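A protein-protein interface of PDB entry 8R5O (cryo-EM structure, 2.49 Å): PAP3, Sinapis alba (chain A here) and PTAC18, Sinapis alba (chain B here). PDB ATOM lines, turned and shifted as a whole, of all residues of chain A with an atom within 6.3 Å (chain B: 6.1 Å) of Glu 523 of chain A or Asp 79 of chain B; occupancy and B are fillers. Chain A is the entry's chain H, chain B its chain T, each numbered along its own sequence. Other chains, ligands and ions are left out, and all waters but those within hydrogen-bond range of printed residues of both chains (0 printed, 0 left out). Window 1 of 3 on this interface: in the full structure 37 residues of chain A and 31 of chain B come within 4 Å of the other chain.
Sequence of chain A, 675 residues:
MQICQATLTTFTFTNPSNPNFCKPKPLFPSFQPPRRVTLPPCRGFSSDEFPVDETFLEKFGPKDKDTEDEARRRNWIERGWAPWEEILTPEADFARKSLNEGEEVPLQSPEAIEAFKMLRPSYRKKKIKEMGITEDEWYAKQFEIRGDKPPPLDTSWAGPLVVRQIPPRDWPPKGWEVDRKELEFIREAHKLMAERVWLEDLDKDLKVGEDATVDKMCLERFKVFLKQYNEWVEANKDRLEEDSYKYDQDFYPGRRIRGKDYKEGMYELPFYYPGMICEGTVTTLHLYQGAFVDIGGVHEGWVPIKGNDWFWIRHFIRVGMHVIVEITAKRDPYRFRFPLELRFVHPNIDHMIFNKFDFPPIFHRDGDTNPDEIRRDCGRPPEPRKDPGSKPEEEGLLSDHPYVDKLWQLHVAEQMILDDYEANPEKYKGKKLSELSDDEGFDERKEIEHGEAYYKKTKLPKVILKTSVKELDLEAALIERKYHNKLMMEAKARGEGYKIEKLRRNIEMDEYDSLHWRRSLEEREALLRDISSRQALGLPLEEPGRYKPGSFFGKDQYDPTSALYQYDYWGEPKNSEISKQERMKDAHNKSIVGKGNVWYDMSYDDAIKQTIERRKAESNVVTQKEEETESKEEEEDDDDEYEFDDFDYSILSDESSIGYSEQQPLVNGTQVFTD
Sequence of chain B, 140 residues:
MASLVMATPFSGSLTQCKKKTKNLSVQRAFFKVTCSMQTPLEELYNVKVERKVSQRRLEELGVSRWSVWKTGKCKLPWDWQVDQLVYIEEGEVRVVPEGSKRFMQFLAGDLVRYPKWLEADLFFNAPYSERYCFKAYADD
OE2 of Glu 523 of chain A sits at hydrogen-bond distance from NE1 of Trp 78 of chain B (3.3 Å).
NH2 of Arg 546 of chain A is in hydrogen-bond range of O of Trp 117 of chain B (3.4 Å).
The guanidinium group (NH2) of Arg 519 of chain A sits close to the indole nitrogen (NE1) of Trp 78 of chain B (3.4 Å).
The backbone NH (N) of Gln 81 of chain B is in hydrogen-bond range of the side-chain carboxylate (OE2) of Glu 523 of chain A (3.3 Å).
The backbone carbonyl oxygen (O) of Ala 120 of chain B lies within hydrogen-bond range of the backbone NH (N) of Trp 78 of chain B, 3.0 Å away.
NE of Arg 518 of chain A is in salt-bridge range of OE2 of Glu 522 of chain A (3.1 Å).
The backbone carbonyl oxygen of Trp 80 of chain B sits at hydrogen-bond distance from the backbone NH of Trp 117 of chain B (2.7 Å).
Among the printed residues, merely in contact across the chains: Leu 527 of chain A with Gln 81 of chain B (3.4 Å), Arg 519 of chain A with Phe 134 of chain B (3.5 Å), Glu 523 of chain A with Phe 134 of chain B (3.7 Å), Glu 523 of chain A with Val 82 of chain B (3.7 Å), Leu 527 of chain A with Val 82 of chain B (3.8 Å), Ala 526 of chain A with Phe 134 of chain B (3.9 Å), Glu 523 of chain A with Asp 79 of chain B (3.9 Å), Glu 522 of chain A with Phe 134 of chain B (3.99 Å) and Ser 520 of chain A with Trp 78 of chain B (3.99 Å).
Arg 518 of chain A touches none of the printed residues of chain B.
Of the printed residues of chain B, Arg 519 of chain A touches Trp 78 (3.3 Å) and Phe 134 (3.5 Å).
Of the printed residues of chain B, Ser 520 of chain A touches Trp 78 (3.99 Å).
Glu 523 of chain A touches five residues of chain B.
Arg 524 of chain A touches none of the printed residues of chain B.
Printed residues of chain B within 4 Å of Leu 527 of chain A: Gln 81 (3.4 Å) and Val 82 (3.8 Å).
Asp 79 of chain B touches just one residue of chain A: Glu 523 (3.9 Å).
Of the printed residues of chain A, Val 82 of chain B touches Glu 523 (3.7 Å) and Leu 527 (3.8 Å).
Of the 11 printed residues of chain B, 6 touch a printed residue of chain A.
Hydrophobic or aromatic side chains of chain B that line the printed part of chain A: Trp 78, Val 82, Trp 117 and Phe 134.
Hydrophobic or aromatic side chains of chain A within 4 Å of the printed part of chain B: Ala 526 and Leu 527.
Among the printed residues, no Asp or Glu carboxylate lies within 4 Å of a Lys or Arg side-chain nitrogen of the other chain.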
ATOM      1  N   ARG A 518      -2.171  32.139  -8.103  1.00  0.00           N
ATOM      2  CA  ARG A 518      -1.156  31.199  -7.640  1.00  0.00           C
ATOM      3  C   ARG A 518      -1.774  29.850  -7.294  1.00  0.00           C
ATOM      4  O   ARG A 518      -1.179  28.799  -7.558  1.00  0.00           O
ATOM      5  CB  ARG A 518      -0.421  31.788  -6.437  1.00  0.00           C
ATOM      6  CG  ARG A 518       0.561  30.850  -5.760  1.00  0.00           C
ATOM      7  CD  ARG A 518       1.708  30.476  -6.674  1.00  0.00           C
ATOM      8  NE  ARG A 518       2.889  30.091  -5.911  1.00  0.00           N
ATOM      9  CZ  ARG A 518       3.987  29.568  -6.439  1.00  0.00           C
ATOM     10  NH1 ARG A 518       4.084  29.331  -7.737  1.00  0.00           N
ATOM     11  NH2 ARG A 518       5.012  29.273  -5.645  1.00  0.00           N
ATOM     12  N   ARG A 519      -2.968  29.862  -6.697  1.00  0.00           N
ATOM     13  CA  ARG A 519      -3.659  28.616  -6.384  1.00  0.00           C
ATOM     14  C   ARG A 519      -4.006  27.841  -7.650  1.00  0.00           C
ATOM     15  O   ARG A 519      -3.852  26.616  -7.698  1.00  0.00           O
ATOM     16  CB  ARG A 519      -4.915  28.916  -5.567  1.00  0.00           C
ATOM     17  CG  ARG A 519      -5.762  27.706  -5.229  1.00  0.00           C
ATOM     18  CD  ARG A 519      -7.015  28.122  -4.483  1.00  0.00           C
ATOM     19  NE  ARG A 519      -7.921  27.003  -4.256  1.00  0.00           N
ATOM     20  CZ  ARG A 519      -8.901  26.655  -5.078  1.00  0.00           C
ATOM     21  NH1 ARG A 519      -9.132  27.318  -6.198  1.00  0.00           N
ATOM     22  NH2 ARG A 519      -9.670  25.617  -4.767  1.00  0.00           N
ATOM     23  N   SER A 520      -4.473  28.538  -8.686  1.00  0.00           N
ATOM     24  CA  SER A 520      -4.782  27.873  -9.947  1.00  0.00           C
ATOM     25  C   SER A 520      -3.524  27.329 -10.612  1.00  0.00           C
ATOM     26  O   SER A 520      -3.549  26.245 -11.204  1.00  0.00           O
ATOM     27  CB  SER A 520      -5.512  28.832 -10.885  1.00  0.00           C
ATOM     28  OG  SER A 520      -6.776  29.196 -10.364  1.00  0.00           O
ATOM     29  N   LEU A 521      -2.418  28.072 -10.534  1.00  0.00           N
ATOM     30  CA  LEU A 521      -1.176  27.620 -11.153  1.00  0.00           C
ATOM     31  C   LEU A 521      -0.663  26.340 -10.506  1.00  0.00           C
ATOM     32  O   LEU A 521      -0.218  25.421 -11.200  1.00  0.00           O
ATOM     33  CB  LEU A 521      -0.118  28.719 -11.069  1.00  0.00           C
ATOM     34  CG  LEU A 521       1.261  28.362 -11.626  1.00  0.00           C
ATOM     35  CD1 LEU A 521       1.191  28.153 -13.129  1.00  0.00           C
ATOM     36  CD2 LEU A 521       2.280  29.430 -11.274  1.00  0.00           C
ATOM     37  N   GLU A 522      -0.717  26.263  -9.174  1.00  0.00           N
ATOM     38  CA  GLU A 522      -0.204  25.084  -8.485  1.00  0.00           C
ATOM     39  C   GLU A 522      -1.067  23.856  -8.745  1.00  0.00           C
ATOM     40  O   GLU A 522      -0.541  22.739  -8.810  1.00  0.00           O
ATOM     41  CB  GLU A 522      -0.092  25.356  -6.986  1.00  0.00           C
ATOM     42  CG  GLU A 522       0.918  26.435  -6.639  1.00  0.00           C
ATOM     43  CD  GLU A 522       1.322  26.413  -5.181  1.00  0.00           C
ATOM     44  OE1 GLU A 522       1.020  25.417  -4.491  1.00  0.00           O
ATOM     45  OE2 GLU A 522       1.947  27.392  -4.725  1.00  0.00           O
ATOM     46  N   GLU A 523      -2.382  24.032  -8.886  1.00  0.00           N
ATOM     47  CA  GLU A 523      -3.232  22.899  -9.236  1.00  0.00           C
ATOM     48  C   GLU A 523      -2.922  22.389 -10.637  1.00  0.00           C
ATOM     49  O   GLU A 523      -2.862  21.176 -10.863  1.00  0.00           O
ATOM     50  CB  GLU A 523      -4.708  23.281  -9.127  1.00  0.00           C
ATOM     51  CG  GLU A 523      -5.646  22.091  -9.250  1.00  0.00           C
ATOM     52  CD  GLU A 523      -7.072  22.490  -9.570  1.00  0.00           C
ATOM     53  OE1 GLU A 523      -7.261  23.458 -10.335  1.00  0.00           O
ATOM     54  OE2 GLU A 523      -8.003  21.835  -9.058  1.00  0.00           O
ATOM     55  N   ARG A 524      -2.728  23.302 -11.591  1.00  0.00           N
ATOM     56  CA  ARG A 524      -2.432  22.894 -12.961  1.00  0.00           C
ATOM     57  C   ARG A 524      -1.093  22.175 -13.049  1.00  0.00           C
ATOM     58  O   ARG A 524      -0.962  21.178 -13.768  1.00  0.00           O
ATOM     59  CB  ARG A 524      -2.449  24.109 -13.887  1.00  0.00           C
ATOM     60  CG  ARG A 524      -2.216  23.776 -15.351  1.00  0.00           C
ATOM     61  CD  ARG A 524      -3.268  22.815 -15.871  1.00  0.00           C
ATOM     62  NE  ARG A 524      -4.617  23.316 -15.643  1.00  0.00           N
ATOM     63  CZ  ARG A 524      -5.261  24.135 -16.463  1.00  0.00           C
ATOM     64  NH1 ARG A 524      -4.711  24.560 -17.589  1.00  0.00           N
ATOM     65  NH2 ARG A 524      -6.486  24.542 -16.144  1.00  0.00           N
ATOM     66  N   GLU A 525      -0.083  22.670 -12.330  1.00  0.00           N
ATOM     67  CA  GLU A 525       1.219  22.012 -12.335  1.00  0.00           C
ATOM     68  C   GLU A 525       1.131  20.608 -11.750  1.00  0.00           C
ATOM     69  O   GLU A 525       1.727  19.666 -12.285  1.00  0.00           O
ATOM     70  CB  GLU A 525       2.235  22.854 -11.567  1.00  0.00           C
ATOM     71  CG  GLU A 525       2.613  24.147 -12.263  1.00  0.00           C
ATOM     72  CD  GLU A 525       3.520  25.019 -11.422  1.00  0.00           C
ATOM     73  OE1 GLU A 525       3.345  25.045 -10.185  1.00  0.00           O
ATOM     74  OE2 GLU A 525       4.415  25.675 -11.996  1.00  0.00           O
ATOM     75  N   ALA A 526       0.392  20.448 -10.651  1.00  0.00           N
ATOM     76  CA  ALA A 526       0.178  19.119 -10.095  1.00  0.00           C
ATOM     77  C   ALA A 526      -0.659  18.253 -11.026  1.00  0.00           C
ATOM     78  O   ALA A 526      -0.451  17.038 -11.090  1.00  0.00           O
ATOM     79  CB  ALA A 526      -0.484  19.220  -8.722  1.00  0.00           C
ATOM     80  N   LEU A 527      -1.603  18.857 -11.750  1.00  0.00           N
ATOM     81  CA  LEU A 527      -2.415  18.097 -12.695  1.00  0.00           C
ATOM     82  C   LEU A 527      -1.568  17.542 -13.833  1.00  0.00           C
ATOM     83  O   LEU A 527      -1.776  16.406 -14.272  1.00  0.00           O
ATOM     84  CB  LEU A 527      -3.541  18.973 -13.243  1.00  0.00           C
ATOM     85  CG  LEU A 527      -4.443  18.340 -14.305  1.00  0.00           C
ATOM     86  CD1 LEU A 527      -5.127  17.097 -13.761  1.00  0.00           C
ATOM     87  CD2 LEU A 527      -5.466  19.343 -14.809  1.00  0.00           C
ATOM     88  N   LEU A 528      -0.610  18.331 -14.325  1.00  0.00           N
ATOM     89  CA  LEU A 528       0.230  17.875 -15.428  1.00  0.00           C
ATOM     90  C   LEU A 528       1.076  16.674 -15.025  1.00  0.00           C
ATOM     91  O   LEU A 528       1.226  15.726 -15.804  1.00  0.00           O
ATOM     92  CB  LEU A 528       1.115  19.021 -15.917  1.00  0.00           C
ATOM     93  CG  LEU A 528       0.374  20.195 -16.561  1.00  0.00           C
ATOM     94  CD1 LEU A 528       1.317  21.361 -16.796  1.00  0.00           C
ATOM     95  CD2 LEU A 528      -0.286  19.768 -17.863  1.00  0.00           C
ATOM     96  N   ARG A 546     -18.721   8.853 -14.929  1.00  0.00           N
ATOM     97  CA  ARG A 546     -18.999  10.183 -15.439  1.00  0.00           C
ATOM     98  C   ARG A 546     -18.590  10.277 -16.909  1.00  0.00           C
ATOM     99  O   ARG A 546     -17.731   9.534 -17.391  1.00  0.00           O
ATOM    100  CB  ARG A 546     -18.257  11.231 -14.606  1.00  0.00           C
ATOM    101  CG  ARG A 546     -18.743  12.659 -14.788  1.00  0.00           C
ATOM    102  CD  ARG A 546     -17.791  13.661 -14.149  1.00  0.00           C
ATOM    103  NE  ARG A 546     -17.654  13.455 -12.712  1.00  0.00           N
ATOM    104  CZ  ARG A 546     -16.927  14.220 -11.909  1.00  0.00           C
ATOM    105  NH1 ARG A 546     -16.261  15.268 -12.367  1.00  0.00           N
ATOM    106  NH2 ARG A 546     -16.862  13.924 -10.615  1.00  0.00           N
ATOM    107  N   PRO B  77     -17.148  28.321  -5.688  1.00  0.00           N
ATOM    108  CA  PRO B  77     -17.374  27.007  -6.299  1.00  0.00           C
ATOM    109  C   PRO B  77     -16.079  26.447  -6.861  1.00  0.00           C
ATOM    110  O   PRO B  77     -15.263  27.173  -7.434  1.00  0.00           O
ATOM    111  CB  PRO B  77     -18.383  27.302  -7.420  1.00  0.00           C
ATOM    112  CG  PRO B  77     -18.586  28.810  -7.423  1.00  0.00           C
ATOM    113  CD  PRO B  77     -17.500  29.415  -6.603  1.00  0.00           C
ATOM    114  N   TRP B  78     -15.886  25.142  -6.693  1.00  0.00           N
ATOM    115  CA  TRP B  78     -14.660  24.526  -7.177  1.00  0.00           C
ATOM    116  C   TRP B  78     -14.880  23.043  -7.433  1.00  0.00           C
ATOM    117  O   TRP B  78     -15.605  22.378  -6.691  1.00  0.00           O
ATOM    118  CB  TRP B  78     -13.511  24.719  -6.180  1.00  0.00           C
ATOM    119  CG  TRP B  78     -12.171  24.510  -6.799  1.00  0.00           C
ATOM    120  CD1 TRP B  78     -11.358  23.427  -6.655  1.00  0.00           C
ATOM    121  CD2 TRP B  78     -11.496  25.406  -7.687  1.00  0.00           C
ATOM    122  NE1 TRP B  78     -10.209  23.598  -7.388  1.00  0.00           N
ATOM    123  CE2 TRP B  78     -10.271  24.805  -8.033  1.00  0.00           C
ATOM    124  CE3 TRP B  78     -11.806  26.662  -8.219  1.00  0.00           C
ATOM    125  CZ2 TRP B  78      -9.357  25.416  -8.886  1.00  0.00           C
ATOM    126  CZ3 TRP B  78     -10.898  27.265  -9.065  1.00  0.00           C
ATOM    127  CH2 TRP B  78      -9.687  26.642  -9.390  1.00  0.00           C
ATOM    128  N   ASP B  79     -14.246  22.539  -8.489  1.00  0.00           N
ATOM    129  CA  ASP B  79     -14.152  21.110  -8.757  1.00  0.00           C
ATOM    130  C   ASP B  79     -12.686  20.712  -8.677  1.00  0.00           C
ATOM    131  O   ASP B  79     -11.872  21.168  -9.485  1.00  0.00           O
ATOM    132  CB  ASP B  79     -14.745  20.755 -10.123  1.00  0.00           C
ATOM    133  CG  ASP B  79     -14.192  21.615 -11.242  1.00  0.00           C
ATOM    134  OD1 ASP B  79     -13.949  22.815 -11.005  1.00  0.00           O
ATOM    135  OD2 ASP B  79     -13.995  21.090 -12.357  1.00  0.00           O
ATOM    136  N   TRP B  80     -12.351  19.870  -7.706  1.00  0.00           N
ATOM    137  CA  TRP B  80     -10.960  19.490  -7.489  1.00  0.00           C
ATOM    138  C   TRP B  80     -10.496  18.539  -8.582  1.00  0.00           C
ATOM    139  O   TRP B  80     -11.088  17.474  -8.785  1.00  0.00           O
ATOM    140  CB  TRP B  80     -10.794  18.853  -6.112  1.00  0.00           C
ATOM    141  CG  TRP B  80     -10.653  19.854  -5.013  1.00  0.00           C
ATOM    142  CD1 TRP B  80      -9.495  20.258  -4.417  1.00  0.00           C
ATOM    143  CD2 TRP B  80     -11.706  20.592  -4.381  1.00  0.00           C
ATOM    144  NE1 TRP B  80      -9.761  21.195  -3.451  1.00  0.00           N
ATOM    145  CE2 TRP B  80     -11.111  21.419  -3.410  1.00  0.00           C
ATOM    146  CE3 TRP B  80     -13.093  20.630  -4.541  1.00  0.00           C
ATOM    147  CZ2 TRP B  80     -11.855  22.273  -2.603  1.00  0.00           C
ATOM    148  CZ3 TRP B  80     -13.829  21.481  -3.741  1.00  0.00           C
ATOM    149  CH2 TRP B  80     -13.210  22.290  -2.782  1.00  0.00           C
ATOM    150  N   GLN B  81      -9.435  18.924  -9.289  1.00  0.00           N
ATOM    151  CA  GLN B  81      -8.840  18.078 -10.312  1.00  0.00           C
ATOM    152  C   GLN B  81      -7.685  17.239  -9.784  1.00  0.00           C
ATOM    153  O   GLN B  81      -7.328  16.239 -10.414  1.00  0.00           O
ATOM    154  CB  GLN B  81      -8.364  18.937 -11.489  1.00  0.00           C
ATOM    155  CG  GLN B  81      -9.502  19.643 -12.208  1.00  0.00           C
ATOM    156  CD  GLN B  81      -9.025  20.703 -13.178  1.00  0.00           C
ATOM    157  OE1 GLN B  81      -7.875  21.138 -13.128  1.00  0.00           O
ATOM    158  NE2 GLN B  81      -9.913  21.130 -14.067  1.00  0.00           N
ATOM    159  N   VAL B  82      -7.101  17.625  -8.651  1.00  0.00           N
ATOM    160  CA  VAL B  82      -6.136  16.816  -7.919  1.00  0.00           C
ATOM    161  C   VAL B  82      -6.446  16.955  -6.433  1.00  0.00           C
ATOM    162  O   VAL B  82      -7.180  17.849  -6.012  1.00  0.00           O
ATOM    163  CB  VAL B  82      -4.674  17.221  -8.209  1.00  0.00           C
ATOM    164  CG1 VAL B  82      -4.255  16.763  -9.596  1.00  0.00           C
ATOM    165  CG2 VAL B  82      -4.505  18.722  -8.073  1.00  0.00           C
ATOM    166  N   TRP B 117     -11.631  14.948  -7.883  1.00  0.00           N
ATOM    167  CA  TRP B 117     -12.953  14.852  -8.512  1.00  0.00           C
ATOM    168  C   TRP B 117     -14.078  15.323  -7.600  1.00  0.00           C
ATOM    169  O   TRP B 117     -15.248  15.059  -7.900  1.00  0.00           O
ATOM    170  CB  TRP B 117     -13.274  13.434  -8.998  1.00  0.00           C
ATOM    171  CG  TRP B 117     -12.316  12.920 -10.020  1.00  0.00           C
ATOM    172  CD1 TRP B 117     -11.754  13.625 -11.038  1.00  0.00           C
ATOM    173  CD2 TRP B 117     -11.793  11.591 -10.111  1.00  0.00           C
ATOM    174  NE1 TRP B 117     -10.919  12.814 -11.769  1.00  0.00           N
ATOM    175  CE2 TRP B 117     -10.925  11.562 -11.217  1.00  0.00           C
ATOM    176  CE3 TRP B 117     -11.977  10.424  -9.367  1.00  0.00           C
ATOM    177  CZ2 TRP B 117     -10.241  10.411 -11.599  1.00  0.00           C
ATOM    178  CZ3 TRP B 117     -11.299   9.282  -9.746  1.00  0.00           C
ATOM    179  CH2 TRP B 117     -10.442   9.283 -10.852  1.00  0.00           C
ATOM    180  N   LEU B 118     -13.771  16.009  -6.504  1.00  0.00           N
ATOM    181  CA  LEU B 118     -14.807  16.553  -5.638  1.00  0.00           C
ATOM    182  C   LEU B 118     -15.326  17.872  -6.193  1.00  0.00           C
ATOM    183  O   LEU B 118     -14.548  18.743  -6.589  1.00  0.00           O
ATOM    184  CB  LEU B 118     -14.266  16.757  -4.223  1.00  0.00           C
ATOM    185  CG  LEU B 118     -15.160  17.528  -3.247  1.00  0.00           C
ATOM    186  CD1 LEU B 118     -16.422  16.742  -2.924  1.00  0.00           C
ATOM    187  CD2 LEU B 118     -14.402  17.881  -1.977  1.00  0.00           C
ATOM    188  N   GLU B 119     -16.649  18.013  -6.225  1.00  0.00           N
ATOM    189  CA  GLU B 119     -17.304  19.251  -6.624  1.00  0.00           C
ATOM    190  C   GLU B 119     -18.105  19.782  -5.445  1.00  0.00           C
ATOM    191  O   GLU B 119     -18.939  19.064  -4.886  1.00  0.00           O
ATOM    192  CB  GLU B 119     -18.214  19.032  -7.835  1.00  0.00           C
ATOM    193  CG  GLU B 119     -17.477  18.613  -9.090  1.00  0.00           C
ATOM    194  CD  GLU B 119     -18.396  18.437 -10.280  1.00  0.00           C
ATOM    195  OE1 GLU B 119     -19.512  17.906 -10.101  1.00  0.00           O
ATOM    196  OE2 GLU B 119     -18.004  18.840 -11.396  1.00  0.00           O
ATOM    197  N   ALA B 120     -17.855  21.034  -5.071  1.00  0.00           N
ATOM    198  CA  ALA B 120     -18.499  21.599  -3.897  1.00  0.00           C
ATOM    199  C   ALA B 120     -18.459  23.117  -3.964  1.00  0.00           C
ATOM    200  O   ALA B 120     -17.714  23.706  -4.752  1.00  0.00           O
ATOM    201  CB  ALA B 120     -17.836  21.109  -2.607  1.00  0.00           C
ATOM    202  N   PHE B 134      -1.175  21.073  -3.323  1.00  0.00           N
ATOM    203  CA  PHE B 134      -1.842  20.116  -4.192  1.00  0.00           C
ATOM    204  C   PHE B 134      -0.965  18.889  -4.391  1.00  0.00           C
ATOM    205  O   PHE B 134       0.248  19.003  -4.590  1.00  0.00           O
ATOM    206  CB  PHE B 134      -2.184  20.753  -5.540  1.00  0.00           C
ATOM    207  CG  PHE B 134      -3.266  21.792  -5.462  1.00  0.00           C
ATOM    208  CD1 PHE B 134      -4.599  21.429  -5.541  1.00  0.00           C
ATOM    209  CD2 PHE B 134      -2.951  23.131  -5.307  1.00  0.00           C
ATOM    210  CE1 PHE B 134      -5.596  22.380  -5.467  1.00  0.00           C
ATOM    211  CE2 PHE B 134      -3.943  24.086  -5.233  1.00  0.00           C
ATOM    212  CZ  PHE B 134      -5.268  23.710  -5.313  1.00  0.00           C
